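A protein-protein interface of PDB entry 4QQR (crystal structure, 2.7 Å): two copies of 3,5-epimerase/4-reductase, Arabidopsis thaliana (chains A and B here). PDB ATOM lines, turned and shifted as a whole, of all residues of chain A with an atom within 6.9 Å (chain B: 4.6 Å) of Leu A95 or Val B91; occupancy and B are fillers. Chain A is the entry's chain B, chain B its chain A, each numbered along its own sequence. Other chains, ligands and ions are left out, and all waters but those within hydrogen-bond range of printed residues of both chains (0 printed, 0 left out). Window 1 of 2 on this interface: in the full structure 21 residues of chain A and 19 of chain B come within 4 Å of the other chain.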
ATOM      1  N   LEU A  46       3.999 -19.058  -6.002  1.00  0.00           N
ATOM      2  CA  LEU A  46       4.106 -17.628  -6.276  1.00  0.00           C
ATOM      3  C   LEU A  46       2.807 -16.910  -5.954  1.00  0.00           C
ATOM      4  O   LEU A  46       2.816 -15.746  -5.551  1.00  0.00           O
ATOM      5  CB  LEU A  46       4.517 -17.371  -7.729  1.00  0.00           C
ATOM      6  CG  LEU A  46       6.004 -17.524  -8.046  1.00  0.00           C
ATOM      7  CD1 LEU A  46       6.406 -16.555  -9.134  1.00  0.00           C
ATOM      8  CD2 LEU A  46       6.863 -17.316  -6.796  1.00  0.00           C
ATOM      9  N   ARG A  49       2.284 -15.008  -0.683  1.00  0.00           N
ATOM     10  CA  ARG A  49       3.450 -14.388  -0.067  1.00  0.00           C
ATOM     11  C   ARG A  49       4.019 -15.184   1.114  1.00  0.00           C
ATOM     12  O   ARG A  49       5.219 -15.125   1.400  1.00  0.00           O
ATOM     13  CB  ARG A  49       3.065 -12.975   0.386  1.00  0.00           C
ATOM     14  CG  ARG A  49       4.096 -12.266   1.237  1.00  0.00           C
ATOM     15  CD  ARG A  49       3.502 -11.040   1.854  1.00  0.00           C
ATOM     16  NE  ARG A  49       4.313  -9.869   1.563  1.00  0.00           N
ATOM     17  CZ  ARG A  49       4.236  -9.162   0.436  1.00  0.00           C
ATOM     18  NH1 ARG A  49       3.386  -9.508  -0.529  1.00  0.00           N
ATOM     19  NH2 ARG A  49       5.019  -8.105   0.272  1.00  0.00           N
ATOM     20  N   THR A  89      -0.239 -16.061 -11.576  1.00  0.00           N
ATOM     21  CA  THR A  89       1.144 -16.531 -11.509  1.00  0.00           C
ATOM     22  C   THR A  89       2.132 -15.557 -12.152  1.00  0.00           C
ATOM     23  O   THR A  89       3.249 -15.359 -11.655  1.00  0.00           O
ATOM     24  CB  THR A  89       1.279 -17.915 -12.185  1.00  0.00           C
ATOM     25  OG1 THR A  89       0.673 -18.910 -11.352  1.00  0.00           O
ATOM     26  CG2 THR A  89       2.728 -18.287 -12.379  1.00  0.00           C
ATOM     27  N   ASN A  90       1.718 -14.951 -13.262  1.00  0.00           N
ATOM     28  CA  ASN A  90       2.610 -14.094 -14.029  1.00  0.00           C
ATOM     29  C   ASN A  90       2.555 -12.679 -13.557  1.00  0.00           C
ATOM     30  O   ASN A  90       3.497 -11.919 -13.762  1.00  0.00           O
ATOM     31  CB  ASN A  90       2.247 -14.105 -15.509  1.00  0.00           C
ATOM     32  CG  ASN A  90       2.862 -15.264 -16.255  1.00  0.00           C
ATOM     33  OD1 ASN A  90       3.356 -16.229 -15.657  1.00  0.00           O
ATOM     34  ND2 ASN A  90       2.829 -15.179 -17.581  1.00  0.00           N
ATOM     35  N   VAL A  91       1.437 -12.312 -12.948  1.00  0.00           N
ATOM     36  CA  VAL A  91       1.274 -10.946 -12.492  1.00  0.00           C
ATOM     37  C   VAL A  91       1.373 -10.877 -10.980  1.00  0.00           C
ATOM     38  O   VAL A  91       2.407 -10.457 -10.464  1.00  0.00           O
ATOM     39  CB  VAL A  91      -0.040 -10.313 -12.984  1.00  0.00           C
ATOM     40  CG1 VAL A  91      -0.062  -8.830 -12.665  1.00  0.00           C
ATOM     41  CG2 VAL A  91      -0.194 -10.546 -14.473  1.00  0.00           C
ATOM     42  N   ALA A  92       0.314 -11.291 -10.279  1.00  0.00           N
ATOM     43  CA  ALA A  92       0.279 -11.240  -8.808  1.00  0.00           C
ATOM     44  C   ALA A  92       1.495 -11.906  -8.196  1.00  0.00           C
ATOM     45  O   ALA A  92       2.203 -11.294  -7.392  1.00  0.00           O
ATOM     46  CB  ALA A  92      -0.983 -11.883  -8.273  1.00  0.00           C
ATOM     47  N   GLY A  93       1.734 -13.151  -8.613  1.00  0.00           N
ATOM     48  CA  GLY A  93       2.820 -13.968  -8.111  1.00  0.00           C
ATOM     49  C   GLY A  93       4.186 -13.375  -8.372  1.00  0.00           C
ATOM     50  O   GLY A  93       5.011 -13.277  -7.469  1.00  0.00           O
ATOM     51  N   THR A  94       4.429 -12.972  -9.609  1.00  0.00           N
ATOM     52  CA  THR A  94       5.707 -12.367  -9.966  1.00  0.00           C
ATOM     53  C   THR A  94       5.963 -11.051  -9.222  1.00  0.00           C
ATOM     54  O   THR A  94       7.076 -10.776  -8.776  1.00  0.00           O
ATOM     55  CB  THR A  94       5.808 -12.168 -11.498  1.00  0.00           C
ATOM     56  OG1 THR A  94       5.702 -13.445 -12.148  1.00  0.00           O
ATOM     57  CG2 THR A  94       7.120 -11.519 -11.877  1.00  0.00           C
ATOM     58  N   LEU A  95       4.921 -10.240  -9.084  1.00  0.00           N
ATOM     59  CA  LEU A  95       5.019  -8.983  -8.350  1.00  0.00           C
ATOM     60  C   LEU A  95       5.252  -9.219  -6.854  1.00  0.00           C
ATOM     61  O   LEU A  95       5.978  -8.473  -6.212  1.00  0.00           O
ATOM     62  CB  LEU A  95       3.771  -8.144  -8.592  1.00  0.00           C
ATOM     63  CG  LEU A  95       3.723  -7.512  -9.987  1.00  0.00           C
ATOM     64  CD1 LEU A  95       2.416  -6.793 -10.226  1.00  0.00           C
ATOM     65  CD2 LEU A  95       4.875  -6.556 -10.149  1.00  0.00           C
ATOM     66  N   THR A  96       4.649 -10.266  -6.304  1.00  0.00           N
ATOM     67  CA  THR A  96       4.838 -10.585  -4.896  1.00  0.00           C
ATOM     68  C   THR A  96       6.275 -11.031  -4.586  1.00  0.00           C
ATOM     69  O   THR A  96       6.896 -10.548  -3.635  1.00  0.00           O
ATOM     70  CB  THR A  96       3.870 -11.682  -4.470  1.00  0.00           C
ATOM     71  OG1 THR A  96       2.526 -11.207  -4.627  1.00  0.00           O
ATOM     72  CG2 THR A  96       4.108 -12.078  -3.020  1.00  0.00           C
ATOM     73  N   LEU A  97       6.796 -11.954  -5.396  1.00  0.00           N
ATOM     74  CA  LEU A  97       8.176 -12.421  -5.270  1.00  0.00           C
ATOM     75  C   LEU A  97       9.151 -11.269  -5.406  1.00  0.00           C
ATOM     76  O   LEU A  97      10.095 -11.152  -4.636  1.00  0.00           O
ATOM     77  CB  LEU A  97       8.495 -13.475  -6.339  1.00  0.00           C
ATOM     78  CG  LEU A  97       9.952 -13.968  -6.406  1.00  0.00           C
ATOM     79  CD1 LEU A  97      10.391 -14.668  -5.127  1.00  0.00           C
ATOM     80  CD2 LEU A  97      10.181 -14.865  -7.610  1.00  0.00           C
ATOM     81  N   ALA A  98       8.916 -10.428  -6.405  1.00  0.00           N
ATOM     82  CA  ALA A  98       9.721  -9.235  -6.614  1.00  0.00           C
ATOM     83  C   ALA A  98       9.766  -8.383  -5.331  1.00  0.00           C
ATOM     84  O   ALA A  98      10.851  -8.003  -4.853  1.00  0.00           O
ATOM     85  CB  ALA A  98       9.177  -8.442  -7.797  1.00  0.00           C
ATOM     86  N   ASP A  99       8.586  -8.126  -4.768  1.00  0.00           N
ATOM     87  CA  ASP A  99       8.430  -7.304  -3.573  1.00  0.00           C
ATOM     88  C   ASP A  99       9.215  -7.854  -2.379  1.00  0.00           C
ATOM     89  O   ASP A  99      10.012  -7.153  -1.754  1.00  0.00           O
ATOM     90  CB  ASP A  99       6.947  -7.234  -3.212  1.00  0.00           C
ATOM     91  CG  ASP A  99       6.673  -6.318  -2.038  1.00  0.00           C
ATOM     92  OD1 ASP A  99       7.031  -6.685  -0.899  1.00  0.00           O
ATOM     93  OD2 ASP A  99       6.091  -5.232  -2.251  1.00  0.00           O
ATOM     94  N   ILE A 100       8.953  -9.114  -2.053  1.00  0.00           N
ATOM     95  CA  ILE A 100       9.675  -9.808  -0.990  1.00  0.00           C
ATOM     96  C   ILE A 100      11.198  -9.761  -1.199  1.00  0.00           C
ATOM     97  O   ILE A 100      11.948  -9.426  -0.272  1.00  0.00           O
ATOM     98  CB  ILE A 100       9.194 -11.280  -0.868  1.00  0.00           C
ATOM     99  CG1 ILE A 100       7.759 -11.341  -0.338  1.00  0.00           C
ATOM    100  CG2 ILE A 100      10.117 -12.080   0.023  1.00  0.00           C
ATOM    101  CD1 ILE A 100       7.082 -12.647  -0.627  1.00  0.00           C
ATOM    102  N   MET A 150       2.657  -5.364 -19.289  1.00  0.00           N
ATOM    103  CA  MET A 150       2.244  -4.743 -18.022  1.00  0.00           C
ATOM    104  C   MET A 150       3.223  -5.061 -16.885  1.00  0.00           C
ATOM    105  O   MET A 150       3.712  -4.152 -16.201  1.00  0.00           O
ATOM    106  CB  MET A 150       0.828  -5.186 -17.615  1.00  0.00           C
ATOM    107  CG  MET A 150      -0.321  -4.622 -18.448  1.00  0.00           C
ATOM    108  SD  MET A 150      -1.926  -5.187 -17.807  1.00  0.00           S
ATOM    109  CE  MET A 150      -3.015  -4.859 -19.175  1.00  0.00           C
ATOM    110  N   VAL A 151       3.515  -6.350 -16.702  1.00  0.00           N
ATOM    111  CA  VAL A 151       4.430  -6.791 -15.653  1.00  0.00           C
ATOM    112  C   VAL A 151       5.826  -6.213 -15.826  1.00  0.00           C
ATOM    113  O   VAL A 151       6.411  -5.724 -14.865  1.00  0.00           O
ATOM    114  CB  VAL A 151       4.501  -8.334 -15.514  1.00  0.00           C
ATOM    115  CG1 VAL A 151       5.543  -8.737 -14.467  1.00  0.00           C
ATOM    116  CG2 VAL A 151       3.145  -8.874 -15.113  1.00  0.00           C
ATOM    117  N   LEU A 154       5.724  -2.548 -14.777  1.00  0.00           N
ATOM    118  CA  LEU A 154       5.688  -2.475 -13.318  1.00  0.00           C
ATOM    119  C   LEU A 154       7.027  -2.839 -12.646  1.00  0.00           C
ATOM    120  O   LEU A 154       7.450  -2.146 -11.709  1.00  0.00           O
ATOM    121  CB  LEU A 154       4.534  -3.319 -12.751  1.00  0.00           C
ATOM    122  CG  LEU A 154       3.105  -2.854 -13.046  1.00  0.00           C
ATOM    123  CD1 LEU A 154       2.067  -3.911 -12.669  1.00  0.00           C
ATOM    124  CD2 LEU A 154       2.835  -1.565 -12.311  1.00  0.00           C
ATOM    125  N   LEU A 155       7.704  -3.885 -13.138  1.00  0.00           N
ATOM    126  CA  LEU A 155       8.929  -4.395 -12.510  1.00  0.00           C
ATOM    127  C   LEU A 155      10.100  -3.404 -12.527  1.00  0.00           C
ATOM    128  O   LEU A 155      11.103  -3.600 -11.833  1.00  0.00           O
ATOM    129  CB  LEU A 155       9.368  -5.725 -13.134  1.00  0.00           C
ATOM    130  CG  LEU A 155       8.642  -6.979 -12.642  1.00  0.00           C
ATOM    131  CD1 LEU A 155       9.292  -8.228 -13.191  1.00  0.00           C
ATOM    132  CD2 LEU A 155       8.608  -6.999 -11.117  1.00  0.00           C
ATOM    133  N   TYR A 158      11.422  -1.801  -9.309  1.00  0.00           N
ATOM    134  CA  TYR A 158      12.058  -2.702  -8.359  1.00  0.00           C
ATOM    135  C   TYR A 158      13.548  -2.794  -8.650  1.00  0.00           C
ATOM    136  O   TYR A 158      13.992  -3.656  -9.419  1.00  0.00           O
ATOM    137  CB  TYR A 158      11.423  -4.093  -8.430  1.00  0.00           C
ATOM    138  CG  TYR A 158       9.966  -4.151  -8.027  1.00  0.00           C
ATOM    139  CD1 TYR A 158       9.584  -4.731  -6.820  1.00  0.00           C
ATOM    140  CD2 TYR A 158       8.967  -3.649  -8.861  1.00  0.00           C
ATOM    141  CE1 TYR A 158       8.253  -4.796  -6.446  1.00  0.00           C
ATOM    142  CE2 TYR A 158       7.633  -3.717  -8.488  1.00  0.00           C
ATOM    143  CZ  TYR A 158       7.290  -4.291  -7.282  1.00  0.00           C
ATOM    144  OH  TYR A 158       5.975  -4.360  -6.910  1.00  0.00           O
ATOM    145  N   THR B  86       2.088   0.899  -3.812  1.00  0.00           N
ATOM    146  CA  THR B  86       0.779   0.865  -4.463  1.00  0.00           C
ATOM    147  C   THR B  86       0.623  -0.391  -5.328  1.00  0.00           C
ATOM    148  O   THR B  86      -0.488  -0.873  -5.563  1.00  0.00           O
ATOM    149  CB  THR B  86       0.516   2.119  -5.310  1.00  0.00           C
ATOM    150  OG1 THR B  86       1.230   3.229  -4.759  1.00  0.00           O
ATOM    151  CG2 THR B  86      -0.977   2.444  -5.320  1.00  0.00           C
ATOM    152  N   ILE B  87       1.744  -0.914  -5.808  1.00  0.00           N
ATOM    153  CA  ILE B  87       1.721  -2.110  -6.637  1.00  0.00           C
ATOM    154  C   ILE B  87       1.350  -3.328  -5.804  1.00  0.00           C
ATOM    155  O   ILE B  87       0.641  -4.219  -6.269  1.00  0.00           O
ATOM    156  CB  ILE B  87       3.080  -2.357  -7.317  1.00  0.00           C
ATOM    157  CG1 ILE B  87       3.318  -1.328  -8.423  1.00  0.00           C
ATOM    158  CG2 ILE B  87       3.143  -3.767  -7.880  1.00  0.00           C
ATOM    159  CD1 ILE B  87       4.692  -1.413  -9.048  1.00  0.00           C
ATOM    160  N   THR B  89      -0.494  -3.398  -3.002  1.00  0.00           N
ATOM    161  CA  THR B  89      -1.875  -3.354  -2.572  1.00  0.00           C
ATOM    162  C   THR B  89      -2.886  -3.149  -3.701  1.00  0.00           C
ATOM    163  O   THR B  89      -3.925  -3.802  -3.709  1.00  0.00           O
ATOM    164  CB  THR B  89      -2.111  -2.357  -1.392  1.00  0.00           C
ATOM    165  OG1 THR B  89      -3.494  -1.973  -1.352  1.00  0.00           O
ATOM    166  CG2 THR B  89      -1.304  -1.126  -1.551  1.00  0.00           C
ATOM    167  N   ASN B  90      -2.600  -2.267  -4.653  1.00  0.00           N
ATOM    168  CA  ASN B  90      -3.595  -1.930  -5.684  1.00  0.00           C
ATOM    169  C   ASN B  90      -3.510  -2.821  -6.914  1.00  0.00           C
ATOM    170  O   ASN B  90      -4.464  -2.928  -7.677  1.00  0.00           O
ATOM    171  CB  ASN B  90      -3.466  -0.468  -6.125  1.00  0.00           C
ATOM    172  CG  ASN B  90      -3.895   0.517  -5.054  1.00  0.00           C
ATOM    173  OD1 ASN B  90      -3.873   0.213  -3.858  1.00  0.00           O
ATOM    174  ND2 ASN B  90      -4.299   1.707  -5.482  1.00  0.00           N
ATOM    175  N   VAL B  91      -2.344  -3.423  -7.119  1.00  0.00           N
ATOM    176  CA  VAL B  91      -2.185  -4.413  -8.154  1.00  0.00           C
ATOM    177  C   VAL B  91      -2.283  -5.821  -7.554  1.00  0.00           C
ATOM    178  O   VAL B  91      -3.324  -6.467  -7.666  1.00  0.00           O
ATOM    179  CB  VAL B  91      -0.873  -4.212  -8.956  1.00  0.00           C
ATOM    180  CG1 VAL B  91      -0.775  -5.221 -10.059  1.00  0.00           C
ATOM    181  CG2 VAL B  91      -0.834  -2.829  -9.564  1.00  0.00           C
ATOM    182  N   ALA B  92      -1.227  -6.289  -6.894  1.00  0.00           N
ATOM    183  CA  ALA B  92      -1.178  -7.708  -6.494  1.00  0.00           C
ATOM    184  C   ALA B  92      -2.264  -8.068  -5.504  1.00  0.00           C
ATOM    185  O   ALA B  92      -2.834  -9.151  -5.576  1.00  0.00           O
ATOM    186  CB  ALA B  92       0.222  -8.130  -5.960  1.00  0.00           C
ATOM    187  N   GLY B  93      -2.549  -7.160  -4.584  1.00  0.00           N
ATOM    188  CA  GLY B  93      -3.581  -7.409  -3.601  1.00  0.00           C
ATOM    189  C   GLY B  93      -4.994  -7.394  -4.164  1.00  0.00           C
ATOM    190  O   GLY B  93      -5.797  -8.261  -3.826  1.00  0.00           O
ATOM    191  N   THR B  94      -5.304  -6.409  -5.006  1.00  0.00           N
ATOM    192  CA  THR B  94      -6.602  -6.347  -5.673  1.00  0.00           C
ATOM    193  C   THR B  94      -6.813  -7.547  -6.612  1.00  0.00           C
ATOM    194  O   THR B  94      -7.914  -8.124  -6.680  1.00  0.00           O
ATOM    195  CB  THR B  94      -6.733  -5.069  -6.511  1.00  0.00           C
ATOM    196  OG1 THR B  94      -6.205  -3.962  -5.781  1.00  0.00           O
ATOM    197  CG2 THR B  94      -8.169  -4.788  -6.842  1.00  0.00           C
ATOM    198  N   LEU B  95      -5.771  -7.903  -7.357  1.00  0.00           N
ATOM    199  CA  LEU B  95      -5.869  -9.052  -8.241  1.00  0.00           C
ATOM    200  C   LEU B  95      -6.048 -10.345  -7.425  1.00  0.00           C
ATOM    201  O   LEU B  95      -6.864 -11.195  -7.790  1.00  0.00           O
ATOM    202  CB  LEU B  95      -4.660  -9.142  -9.183  1.00  0.00           C
ATOM    203  CG  LEU B  95      -4.697  -8.446 -10.555  1.00  0.00           C
ATOM    204  CD1 LEU B  95      -6.108  -8.245 -11.051  1.00  0.00           C
ATOM    205  CD2 LEU B  95      -3.977  -7.140 -10.544  1.00  0.00           C
ATOM    206  N   THR B 147      -0.948   2.684 -13.762  1.00  0.00           N
ATOM    207  CA  THR B 147      -1.150   1.532 -12.892  1.00  0.00           C
ATOM    208  C   THR B 147      -2.630   1.186 -12.702  1.00  0.00           C
ATOM    209  O   THR B 147      -3.027   0.013 -12.832  1.00  0.00           O
ATOM    210  CB  THR B 147      -0.459   1.731 -11.536  1.00  0.00           C
ATOM    211  OG1 THR B 147       0.943   1.941 -11.748  1.00  0.00           O
ATOM    212  CG2 THR B 147      -0.639   0.516 -10.664  1.00  0.00           C
ATOM    213  N   VAL B 151      -4.616  -2.415 -13.822  1.00  0.00           N
ATOM    214  CA  VAL B 151      -5.498  -3.218 -12.967  1.00  0.00           C
ATOM    215  C   VAL B 151      -6.899  -3.258 -13.534  1.00  0.00           C
ATOM    216  O   VAL B 151      -7.490  -4.338 -13.633  1.00  0.00           O
ATOM    217  CB  VAL B 151      -5.553  -2.719 -11.500  1.00  0.00           C
ATOM    218  CG1 VAL B 151      -6.612  -3.481 -10.718  1.00  0.00           C
ATOM    219  CG2 VAL B 151      -4.195  -2.879 -10.845  1.00  0.00           C
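N of Ala B92 sits at hydrogen-bond distance from O of Ile B87, 2.9 Å away.
OG1 of Thr A96 is in hydrogen-bond range of O of Ala A92.
Among the printed residues, pairs that only touch across the chains: Tyr A158 with Ile B87 (3.1 Å), Leu A95 with Val B91 (3.6 Å), Leu A154 with Ile B87 (3.8 Å), Leu A95 with Ile B87 (3.9 Å) and Ala A92 with Ala B92 (3.998 Å).
Val A91 touches none of the printed residues of chain B.
Of the printed residues of chain B, Ala A92 touches Ala B92 (3.998 Å).
Of chain B, only Ile B87 (3.9 Å) and Val B91 (3.6 Å) come within 4 Å of Leu A95.
Of the printed residues of chain B, Leu A154 touches Ile B87.
Of the printed residues of chain B, Tyr A158 touches Ile B87 (3.1 Å).
Of the printed residues of chain A, Ile B87 touches Leu A95 (3.9 Å), Leu A154 (3.8 Å) and Tyr A158 (3.1 Å).
Val B91 touches just one residue of chain A: Leu A95 (3.6 Å).
Printed residues of chain A within 4 Å of Ala B92: Ala A92 (3.998 Å).
The nearest residue of chain B that does not touch Leu A95 is Ala B92 (4.4 Å).
The nearest printed residue of chain B that does not touch Leu A154 is Thr B147 (4.02 Å).
Of the 11 printed residues of chain B, 3 touch a printed residue of chain A.
Of the 19 printed residues of chain A, 4 touch a printed residue of chain B.
Among the printed residues, no Asp or Glu carboxylate lies within 4 Å of a Lys or Arg side-chain nitrogen of the other chain.
Ala B92 touches its own counterpart, Ala A92.
Leu A95 touches Val B91, but with the chains exchanged Val A91 does not touch Leu B95 (4.8 Å).
Of the 5 pairs that touch across the chains among the printed residues, 1 has its exchanged pair printed and touching as well.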
